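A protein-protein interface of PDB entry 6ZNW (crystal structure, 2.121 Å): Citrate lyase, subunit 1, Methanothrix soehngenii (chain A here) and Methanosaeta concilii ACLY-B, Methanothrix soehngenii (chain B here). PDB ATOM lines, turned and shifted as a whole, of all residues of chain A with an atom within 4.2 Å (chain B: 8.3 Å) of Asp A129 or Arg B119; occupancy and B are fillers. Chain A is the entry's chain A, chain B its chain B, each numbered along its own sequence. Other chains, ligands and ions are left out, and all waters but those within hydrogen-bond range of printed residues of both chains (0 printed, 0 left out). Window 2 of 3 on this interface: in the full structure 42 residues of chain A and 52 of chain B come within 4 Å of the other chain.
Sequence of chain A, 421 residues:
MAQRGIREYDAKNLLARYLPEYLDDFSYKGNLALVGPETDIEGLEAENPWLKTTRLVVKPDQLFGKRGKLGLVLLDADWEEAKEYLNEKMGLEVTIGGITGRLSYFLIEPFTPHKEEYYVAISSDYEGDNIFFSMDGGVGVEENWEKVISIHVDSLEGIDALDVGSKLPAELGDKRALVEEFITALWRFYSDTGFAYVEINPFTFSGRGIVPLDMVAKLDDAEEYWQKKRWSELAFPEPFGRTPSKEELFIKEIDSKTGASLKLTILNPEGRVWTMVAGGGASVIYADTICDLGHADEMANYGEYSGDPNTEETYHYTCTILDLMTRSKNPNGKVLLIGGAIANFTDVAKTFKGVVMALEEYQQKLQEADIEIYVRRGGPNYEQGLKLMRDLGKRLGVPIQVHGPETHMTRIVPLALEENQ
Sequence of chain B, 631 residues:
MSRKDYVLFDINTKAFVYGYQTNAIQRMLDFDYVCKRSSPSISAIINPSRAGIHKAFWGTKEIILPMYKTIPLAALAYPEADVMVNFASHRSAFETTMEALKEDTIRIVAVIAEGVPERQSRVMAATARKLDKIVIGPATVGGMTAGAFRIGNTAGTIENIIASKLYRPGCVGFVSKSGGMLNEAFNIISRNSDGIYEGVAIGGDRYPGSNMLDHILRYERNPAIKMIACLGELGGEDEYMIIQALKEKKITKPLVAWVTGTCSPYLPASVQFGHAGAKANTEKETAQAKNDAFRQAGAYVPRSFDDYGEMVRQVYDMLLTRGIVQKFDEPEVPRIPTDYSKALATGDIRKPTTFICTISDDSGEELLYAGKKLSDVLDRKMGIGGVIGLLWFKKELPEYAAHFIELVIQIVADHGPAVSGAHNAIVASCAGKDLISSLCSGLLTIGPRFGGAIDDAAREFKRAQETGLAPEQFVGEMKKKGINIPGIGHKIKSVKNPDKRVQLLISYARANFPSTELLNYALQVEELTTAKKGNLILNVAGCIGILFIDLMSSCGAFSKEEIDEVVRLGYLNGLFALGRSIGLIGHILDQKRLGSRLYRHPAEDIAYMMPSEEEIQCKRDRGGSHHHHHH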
ATOM      1  N   SER A 123      33.041  25.719  11.312  1.00  0.00           N
ATOM      2  CA  SER A 123      33.013  24.388  10.727  1.00  0.00           C
ATOM      3  C   SER A 123      32.956  23.381  11.886  1.00  0.00           C
ATOM      4  O   SER A 123      33.255  23.744  13.022  1.00  0.00           O
ATOM      5  CB  SER A 123      34.278  24.158   9.908  1.00  0.00           C
ATOM      6  OG  SER A 123      34.047  23.223   8.867  1.00  0.00           O
ATOM      7  N   SER A 124      32.582  22.124  11.613  1.00  0.00           N
ATOM      8  CA  SER A 124      32.494  21.127  12.680  1.00  0.00           C
ATOM      9  C   SER A 124      33.446  19.956  12.517  1.00  0.00           C
ATOM     10  O   SER A 124      33.819  19.603  11.404  1.00  0.00           O
ATOM     11  CB  SER A 124      31.061  20.636  12.826  1.00  0.00           C
ATOM     12  OG  SER A 124      30.179  21.700  13.140  1.00  0.00           O
ATOM     13  N   GLY A 128      33.155  18.536  18.235  1.00  0.00           N
ATOM     14  CA  GLY A 128      32.361  19.747  18.362  1.00  0.00           C
ATOM     15  C   GLY A 128      32.486  20.671  17.172  1.00  0.00           C
ATOM     16  O   GLY A 128      32.635  20.221  16.039  1.00  0.00           O
ATOM     17  N   ASP A 129      32.421  21.978  17.426  1.00  0.00           N
ATOM     18  CA  ASP A 129      32.517  23.001  16.386  1.00  0.00           C
ATOM     19  C   ASP A 129      33.793  23.826  16.563  1.00  0.00           C
ATOM     20  O   ASP A 129      34.234  24.052  17.682  1.00  0.00           O
ATOM     21  CB  ASP A 129      31.282  23.918  16.429  1.00  0.00           C
ATOM     22  CG  ASP A 129      29.962  23.165  16.514  1.00  0.00           C
ATOM     23  OD1 ASP A 129      29.759  22.227  15.708  1.00  0.00           O
ATOM     24  OD2 ASP A 129      29.134  23.512  17.389  1.00  0.00           O
ATOM     25  N   ASN A 130      34.389  24.271  15.463  1.00  0.00           N
ATOM     26  CA  ASN A 130      35.599  25.079  15.497  1.00  0.00           C
ATOM     27  C   ASN A 130      35.341  26.449  14.886  1.00  0.00           C
ATOM     28  O   ASN A 130      34.827  26.552  13.772  1.00  0.00           O
ATOM     29  CB  ASN A 130      36.746  24.380  14.768  1.00  0.00           C
ATOM     30  CG  ASN A 130      37.123  23.049  15.369  1.00  0.00           C
ATOM     31  OD1 ASN A 130      37.489  22.953  16.544  1.00  0.00           O
ATOM     32  ND2 ASN A 130      37.041  21.992  14.572  1.00  0.00           N
ATOM     33  N   ILE A 151      39.231  28.208  17.845  1.00  0.00           N
ATOM     34  CA  ILE A 151      38.589  28.013  19.140  1.00  0.00           C
ATOM     35  C   ILE A 151      37.586  26.866  19.064  1.00  0.00           C
ATOM     36  O   ILE A 151      36.640  26.907  18.277  1.00  0.00           O
ATOM     37  CB  ILE A 151      38.001  29.307  19.755  1.00  0.00           C
ATOM     38  CG1 ILE A 151      36.779  29.831  18.992  1.00  0.00           C
ATOM     39  CG2 ILE A 151      39.079  30.396  19.906  1.00  0.00           C
ATOM     40  CD1 ILE A 151      36.017  30.861  19.783  1.00  0.00           C
ATOM     41  N   HIS A 152      37.827  25.814  19.848  1.00  0.00           N
ATOM     42  CA  HIS A 152      36.971  24.637  19.839  1.00  0.00           C
ATOM     43  C   HIS A 152      35.844  24.717  20.859  1.00  0.00           C
ATOM     44  O   HIS A 152      36.078  24.971  22.035  1.00  0.00           O
ATOM     45  CB  HIS A 152      37.796  23.357  20.035  1.00  0.00           C
ATOM     46  CG  HIS A 152      36.967  22.112  19.996  1.00  0.00           C
ATOM     47  ND1 HIS A 152      36.512  21.586  18.801  1.00  0.00           N
ATOM     48  CD2 HIS A 152      36.510  21.346  21.014  1.00  0.00           C
ATOM     49  CE1 HIS A 152      35.812  20.513  19.126  1.00  0.00           C
ATOM     50  NE2 HIS A 152      35.777  20.332  20.448  1.00  0.00           N
ATOM     51  N   VAL A 153      34.622  24.466  20.395  1.00  0.00           N
ATOM     52  CA  VAL A 153      33.413  24.462  21.206  1.00  0.00           C
ATOM     53  C   VAL A 153      32.934  23.012  21.305  1.00  0.00           C
ATOM     54  O   VAL A 153      32.541  22.422  20.299  1.00  0.00           O
ATOM     55  CB  VAL A 153      32.317  25.368  20.597  1.00  0.00           C
ATOM     56  CG1 VAL A 153      31.147  25.512  21.554  1.00  0.00           C
ATOM     57  CG2 VAL A 153      32.869  26.739  20.219  1.00  0.00           C
ATOM     58  N   SER A 155      30.733  19.680  21.942  1.00  0.00           N
ATOM     59  CA  SER A 155      29.356  19.304  21.601  1.00  0.00           C
ATOM     60  C   SER A 155      28.390  19.319  22.782  1.00  0.00           C
ATOM     61  O   SER A 155      27.241  19.734  22.632  1.00  0.00           O
ATOM     62  CB  SER A 155      29.326  17.927  20.943  1.00  0.00           C
ATOM     63  OG  SER A 155      29.731  17.977  19.586  1.00  0.00           O
ATOM     64  N   TRP A 187      28.046  31.633  16.575  1.00  0.00           N
ATOM     65  CA  TRP A 187      28.059  30.204  16.900  1.00  0.00           C
ATOM     66  C   TRP A 187      26.653  29.743  17.260  1.00  0.00           C
ATOM     67  O   TRP A 187      26.246  28.662  16.850  1.00  0.00           O
ATOM     68  CB  TRP A 187      29.031  29.866  18.050  1.00  0.00           C
ATOM     69  CG  TRP A 187      28.989  28.409  18.425  1.00  0.00           C
ATOM     70  CD1 TRP A 187      29.587  27.377  17.765  1.00  0.00           C
ATOM     71  CD2 TRP A 187      28.181  27.811  19.453  1.00  0.00           C
ATOM     72  NE1 TRP A 187      29.243  26.179  18.346  1.00  0.00           N
ATOM     73  CE2 TRP A 187      28.375  26.416  19.380  1.00  0.00           C
ATOM     74  CE3 TRP A 187      27.306  28.317  20.419  1.00  0.00           C
ATOM     75  CZ2 TRP A 187      27.756  25.533  20.263  1.00  0.00           C
ATOM     76  CZ3 TRP A 187      26.709  27.439  21.302  1.00  0.00           C
ATOM     77  CH2 TRP A 187      26.931  26.065  21.213  1.00  0.00           C
ATOM     78  N   TYR A 190      24.729  29.509  14.133  1.00  0.00           N
ATOM     79  CA  TYR A 190      25.224  28.337  13.419  1.00  0.00           C
ATOM     80  C   TYR A 190      24.560  27.068  13.990  1.00  0.00           C
ATOM     81  O   TYR A 190      24.005  26.264  13.242  1.00  0.00           O
ATOM     82  CB  TYR A 190      26.769  28.284  13.565  1.00  0.00           C
ATOM     83  CG  TYR A 190      27.456  27.052  13.016  1.00  0.00           C
ATOM     84  CD1 TYR A 190      27.930  27.020  11.712  1.00  0.00           C
ATOM     85  CD2 TYR A 190      27.746  25.969  13.834  1.00  0.00           C
ATOM     86  CE1 TYR A 190      28.574  25.897  11.204  1.00  0.00           C
ATOM     87  CE2 TYR A 190      28.410  24.850  13.345  1.00  0.00           C
ATOM     88  CZ  TYR A 190      28.827  24.818  12.029  1.00  0.00           C
ATOM     89  OH  TYR A 190      29.478  23.710  11.543  1.00  0.00           O
ATOM     90  N   SER A 191      24.578  26.933  15.322  1.00  0.00           N
ATOM     91  CA  SER A 191      24.061  25.796  16.069  1.00  0.00           C
ATOM     92  C   SER A 191      22.541  25.631  16.046  1.00  0.00           C
ATOM     93  O   SER A 191      22.055  24.500  16.020  1.00  0.00           O
ATOM     94  CB  SER A 191      24.560  25.846  17.512  1.00  0.00           C
ATOM     95  OG  SER A 191      23.900  26.831  18.289  1.00  0.00           O
ATOM     96  N   GLU A 223      18.453  18.821   8.542  1.00  0.00           N
ATOM     97  CA  GLU A 223      17.857  19.701   9.552  1.00  0.00           C
ATOM     98  C   GLU A 223      16.476  20.248   9.157  1.00  0.00           C
ATOM     99  O   GLU A 223      15.799  20.825  10.003  1.00  0.00           O
ATOM    100  CB  GLU A 223      18.795  20.895   9.828  1.00  0.00           C
ATOM    101  CG  GLU A 223      20.060  20.526  10.580  1.00  0.00           C
ATOM    102  CD  GLU A 223      19.990  20.706  12.085  1.00  0.00           C
ATOM    103  OE1 GLU A 223      21.026  20.481  12.752  1.00  0.00           O
ATOM    104  OE2 GLU A 223      18.911  21.083  12.597  1.00  0.00           O
ATOM    105  N   PHE B  94      17.158  10.695  17.588  1.00  0.00           N
ATOM    106  CA  PHE B  94      17.992  11.358  18.595  1.00  0.00           C
ATOM    107  C   PHE B  94      17.429  11.236  20.003  1.00  0.00           C
ATOM    108  O   PHE B  94      18.139  10.753  20.874  1.00  0.00           O
ATOM    109  CB  PHE B  94      18.247  12.834  18.244  1.00  0.00           C
ATOM    110  CG  PHE B  94      19.036  13.627  19.262  1.00  0.00           C
ATOM    111  CD1 PHE B  94      20.414  13.540  19.312  1.00  0.00           C
ATOM    112  CD2 PHE B  94      18.403  14.498  20.132  1.00  0.00           C
ATOM    113  CE1 PHE B  94      21.143  14.293  20.225  1.00  0.00           C
ATOM    114  CE2 PHE B  94      19.134  15.251  21.046  1.00  0.00           C
ATOM    115  CZ  PHE B  94      20.500  15.149  21.080  1.00  0.00           C
ATOM    116  N   VAL B 116      19.373  11.775   9.802  1.00  0.00           N
ATOM    117  CA  VAL B 116      19.553  12.357  11.127  1.00  0.00           C
ATOM    118  C   VAL B 116      20.535  13.542  11.018  1.00  0.00           C
ATOM    119  O   VAL B 116      21.616  13.395  10.437  1.00  0.00           O
ATOM    120  CB  VAL B 116      20.062  11.291  12.132  1.00  0.00           C
ATOM    121  CG1 VAL B 116      20.377  11.914  13.492  1.00  0.00           C
ATOM    122  CG2 VAL B 116      19.063  10.138  12.274  1.00  0.00           C
ATOM    123  N   PRO B 117      20.179  14.736  11.555  1.00  0.00           N
ATOM    124  CA  PRO B 117      21.095  15.885  11.480  1.00  0.00           C
ATOM    125  C   PRO B 117      22.505  15.594  11.982  1.00  0.00           C
ATOM    126  O   PRO B 117      22.684  14.788  12.900  1.00  0.00           O
ATOM    127  CB  PRO B 117      20.417  16.939  12.364  1.00  0.00           C
ATOM    128  CG  PRO B 117      18.996  16.597  12.334  1.00  0.00           C
ATOM    129  CD  PRO B 117      18.929  15.096  12.247  1.00  0.00           C
ATOM    130  N   GLU B 118      23.500  16.239  11.365  1.00  0.00           N
ATOM    131  CA  GLU B 118      24.897  16.062  11.728  1.00  0.00           C
ATOM    132  C   GLU B 118      25.156  16.489  13.173  1.00  0.00           C
ATOM    133  O   GLU B 118      25.918  15.821  13.876  1.00  0.00           O
ATOM    134  CB  GLU B 118      25.819  16.781  10.721  1.00  0.00           C
ATOM    135  CG  GLU B 118      25.848  16.066   9.380  1.00  0.00           C
ATOM    136  CD  GLU B 118      26.436  16.801   8.191  1.00  0.00           C
ATOM    137  OE1 GLU B 118      27.064  17.864   8.395  1.00  0.00           O
ATOM    138  OE2 GLU B 118      26.262  16.310   7.050  1.00  0.00           O
ATOM    139  N   ARG B 119      24.471  17.556  13.633  1.00  0.00           N
ATOM    140  CA  ARG B 119      24.603  18.052  15.002  1.00  0.00           C
ATOM    141  C   ARG B 119      24.103  17.031  16.020  1.00  0.00           C
ATOM    142  O   ARG B 119      24.753  16.823  17.040  1.00  0.00           O
ATOM    143  CB  ARG B 119      23.910  19.418  15.189  1.00  0.00           C
ATOM    144  CG  ARG B 119      23.937  19.868  16.644  1.00  0.00           C
ATOM    145  CD  ARG B 119      23.676  21.324  16.906  1.00  0.00           C
ATOM    146  NE  ARG B 119      23.760  21.582  18.344  1.00  0.00           N
ATOM    147  CZ  ARG B 119      24.889  21.851  18.997  1.00  0.00           C
ATOM    148  NH1 ARG B 119      24.869  22.063  20.306  1.00  0.00           N
ATOM    149  NH2 ARG B 119      26.044  21.920  18.343  1.00  0.00           N
ATOM    150  N   GLN B 120      22.969  16.397  15.745  1.00  0.00           N
ATOM    151  CA  GLN B 120      22.387  15.375  16.615  1.00  0.00           C
ATOM    152  C   GLN B 120      23.333  14.178  16.746  1.00  0.00           C
ATOM    153  O   GLN B 120      23.568  13.712  17.855  1.00  0.00           O
ATOM    154  CB  GLN B 120      21.024  14.934  16.070  1.00  0.00           C
ATOM    155  CG  GLN B 120      19.916  15.944  16.330  1.00  0.00           C
ATOM    156  CD  GLN B 120      18.586  15.514  15.767  1.00  0.00           C
ATOM    157  OE1 GLN B 120      18.343  14.337  15.482  1.00  0.00           O
ATOM    158  NE2 GLN B 120      17.687  16.465  15.587  1.00  0.00           N
ATOM    159  N   SER B 121      23.918  13.728  15.625  1.00  0.00           N
ATOM    160  CA  SER B 121      24.883  12.634  15.614  1.00  0.00           C
ATOM    161  C   SER B 121      26.146  12.997  16.400  1.00  0.00           C
ATOM    162  O   SER B 121      26.666  12.147  17.122  1.00  0.00           O
ATOM    163  CB  SER B 121      25.232  12.251  14.184  1.00  0.00           C
ATOM    164  OG  SER B 121      24.083  11.756  13.521  1.00  0.00           O
ATOM    165  N   ARG B 122      26.610  14.268  16.303  1.00  0.00           N
ATOM    166  CA  ARG B 122      27.773  14.748  17.054  1.00  0.00           C
ATOM    167  C   ARG B 122      27.483  14.647  18.562  1.00  0.00           C
ATOM    168  O   ARG B 122      28.336  14.200  19.329  1.00  0.00           O
ATOM    169  CB  ARG B 122      28.124  16.218  16.689  1.00  0.00           C
ATOM    170  CG  ARG B 122      28.923  16.404  15.392  1.00  0.00           C
ATOM    171  CD  ARG B 122      29.485  17.820  15.197  1.00  0.00           C
ATOM    172  NE  ARG B 122      28.467  18.814  14.838  1.00  0.00           N
ATOM    173  CZ  ARG B 122      28.030  19.032  13.598  1.00  0.00           C
ATOM    174  NH1 ARG B 122      27.105  19.955  13.366  1.00  0.00           N
ATOM    175  NH2 ARG B 122      28.519  18.333  12.581  1.00  0.00           N
ATOM    176  N   VAL B 123      26.276  15.057  18.983  1.00  0.00           N
ATOM    177  CA  VAL B 123      25.872  15.024  20.390  1.00  0.00           C
ATOM    178  C   VAL B 123      25.707  13.579  20.893  1.00  0.00           C
ATOM    179  O   VAL B 123      26.082  13.293  22.028  1.00  0.00           O
ATOM    180  CB  VAL B 123      24.622  15.899  20.650  1.00  0.00           C
ATOM    181  CG1 VAL B 123      24.067  15.683  22.055  1.00  0.00           C
ATOM    182  CG2 VAL B 123      24.932  17.368  20.408  1.00  0.00           C
ATOM    183  N   MET B 124      25.216  12.665  20.040  1.00  0.00           N
ATOM    184  CA  MET B 124      25.057  11.255  20.409  1.00  0.00           C
ATOM    185  C   MET B 124      26.418  10.599  20.587  1.00  0.00           C
ATOM    186  O   MET B 124      26.620   9.877  21.559  1.00  0.00           O
ATOM    187  CB  MET B 124      24.232  10.485  19.360  1.00  0.00           C
ATOM    188  CG  MET B 124      22.775  10.851  19.360  1.00  0.00           C
ATOM    189  SD  MET B 124      21.705   9.785  18.350  1.00  0.00           S
ATOM    190  CE  MET B 124      22.172  10.265  16.717  1.00  0.00           C
ATOM    191  N   ALA B 125      27.358  10.880  19.660  1.00  0.00           N
ATOM    192  CA  ALA B 125      28.726  10.356  19.694  1.00  0.00           C
ATOM    193  C   ALA B 125      29.459  10.831  20.943  1.00  0.00           C
ATOM    194  O   ALA B 125      30.077  10.015  21.617  1.00  0.00           O
ATOM    195  CB  ALA B 125      29.494  10.774  18.442  1.00  0.00           C
ATOM    196  N   ALA B 126      29.350  12.127  21.283  1.00  0.00           N
ATOM    197  CA  ALA B 126      30.004  12.673  22.461  1.00  0.00           C
ATOM    198  C   ALA B 126      29.387  12.122  23.749  1.00  0.00           C
ATOM    199  O   ALA B 126      30.121  11.867  24.714  1.00  0.00           O
ATOM    200  CB  ALA B 126      29.942  14.199  22.442  1.00  0.00           C
ATOM    201  N   TYR B 207      29.381  12.438  10.331  1.00  0.00           N
ATOM    202  CA  TYR B 207      29.661  12.451  11.774  1.00  0.00           C
ATOM    203  C   TYR B 207      28.976  11.229  12.397  1.00  0.00           C
ATOM    204  O   TYR B 207      27.809  11.308  12.774  1.00  0.00           O
ATOM    205  CB  TYR B 207      29.187  13.755  12.440  1.00  0.00           C
ATOM    206  CG  TYR B 207      29.879  14.963  11.857  1.00  0.00           C
ATOM    207  CD1 TYR B 207      31.166  15.308  12.249  1.00  0.00           C
ATOM    208  CD2 TYR B 207      29.285  15.708  10.851  1.00  0.00           C
ATOM    209  CE1 TYR B 207      31.837  16.376  11.664  1.00  0.00           C
ATOM    210  CE2 TYR B 207      29.940  16.786  10.267  1.00  0.00           C
ATOM    211  CZ  TYR B 207      31.219  17.113  10.672  1.00  0.00           C
ATOM    212  OH  TYR B 207      31.877  18.162  10.080  1.00  0.00           O
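The backbone carbonyl oxygen (O) of Ser A124 lies within hydrogen-bond range of the side-chain hydroxyl (OH) of Tyr B207.
The guanidinium group (NH2) of Arg B119 is in salt-bridge range of the side-chain carboxylate (OD2) of Asp A129 (3.6 Å).
NE of Arg B122 lies within salt-bridge range of OD1 of Asp A129, 3.8 Å away.
Among the printed residues, pairs that only touch across the chains: Ser A124 with Arg B122 (3.4 Å), Ser A155 with Arg B122 (3.8 Å), Ser A155 with Val B123 (3.98 Å), Ser A191 with Arg B119 (3.7 Å), Glu A223 with Pro B117 (3.6 Å) and Glu A223 with Arg B119 (3.9 Å).
Asp A129 touches just these residues of chain B: Arg B119 (3.6 Å) and Arg B122 (3.8 Å).
No residue of chain B comes within 4 Å of Gly A128.
No residue of chain B comes within 4 Å of Asn A130.
Of the printed residues of chain B, Ser A124 touches Arg B122 and Tyr B207.
Printed residues of chain A within 4 Å of Arg B122: Ser A124 (3.4 Å), Asp A129 (3.8 Å) and Ser A155 (3.8 Å).
Met B124 touches none of the printed residues of chain A.
The nearest residue of chain A that does not touch Arg B119 is Ser A155 (4.1 Å).
The nearest printed residue of chain B that does not touch Glu A223 is Glu B118 (5.1 Å).
Of the 13 printed residues of chain A, 5 touch a printed residue of chain B.
Of the 13 printed residues of chain B, 5 touch a printed residue of chain A.
Printed residues of chain B that touch a printed residue of chain A: Pro B117, Arg B119, Arg B122, Val B123 and Tyr B207.
Among the printed residues, 9 pairs touch across the chains.
The side-chain hydroxyl (OG) of Ser A124 is in hydrogen-bond range of the side-chain carboxylate (OD1) of Asp A129 (2.7 Å).
OG of Ser A124 sits at hydrogen-bond distance from OH of Tyr A190, at 2.7 Å.
The backbone NH of Val A153 lies within hydrogen-bond range of the backbone carbonyl oxygen of Asp A129 (2.8 Å).
The side-chain carboxylate (OD2) of Asp A129 is in hydrogen-bond range of the indole nitrogen (NE1) of Trp A187 (2.8 Å).
The side-chain hydroxyl (OG) of Ser A191 sits at hydrogen-bond distance from the backbone carbonyl oxygen (O) of Trp A187.
The backbone carbonyl oxygen (O) of Pro B117 sits at hydrogen-bond distance from the side-chain hydroxyl (OG) of Ser B121, 3.4 Å away.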
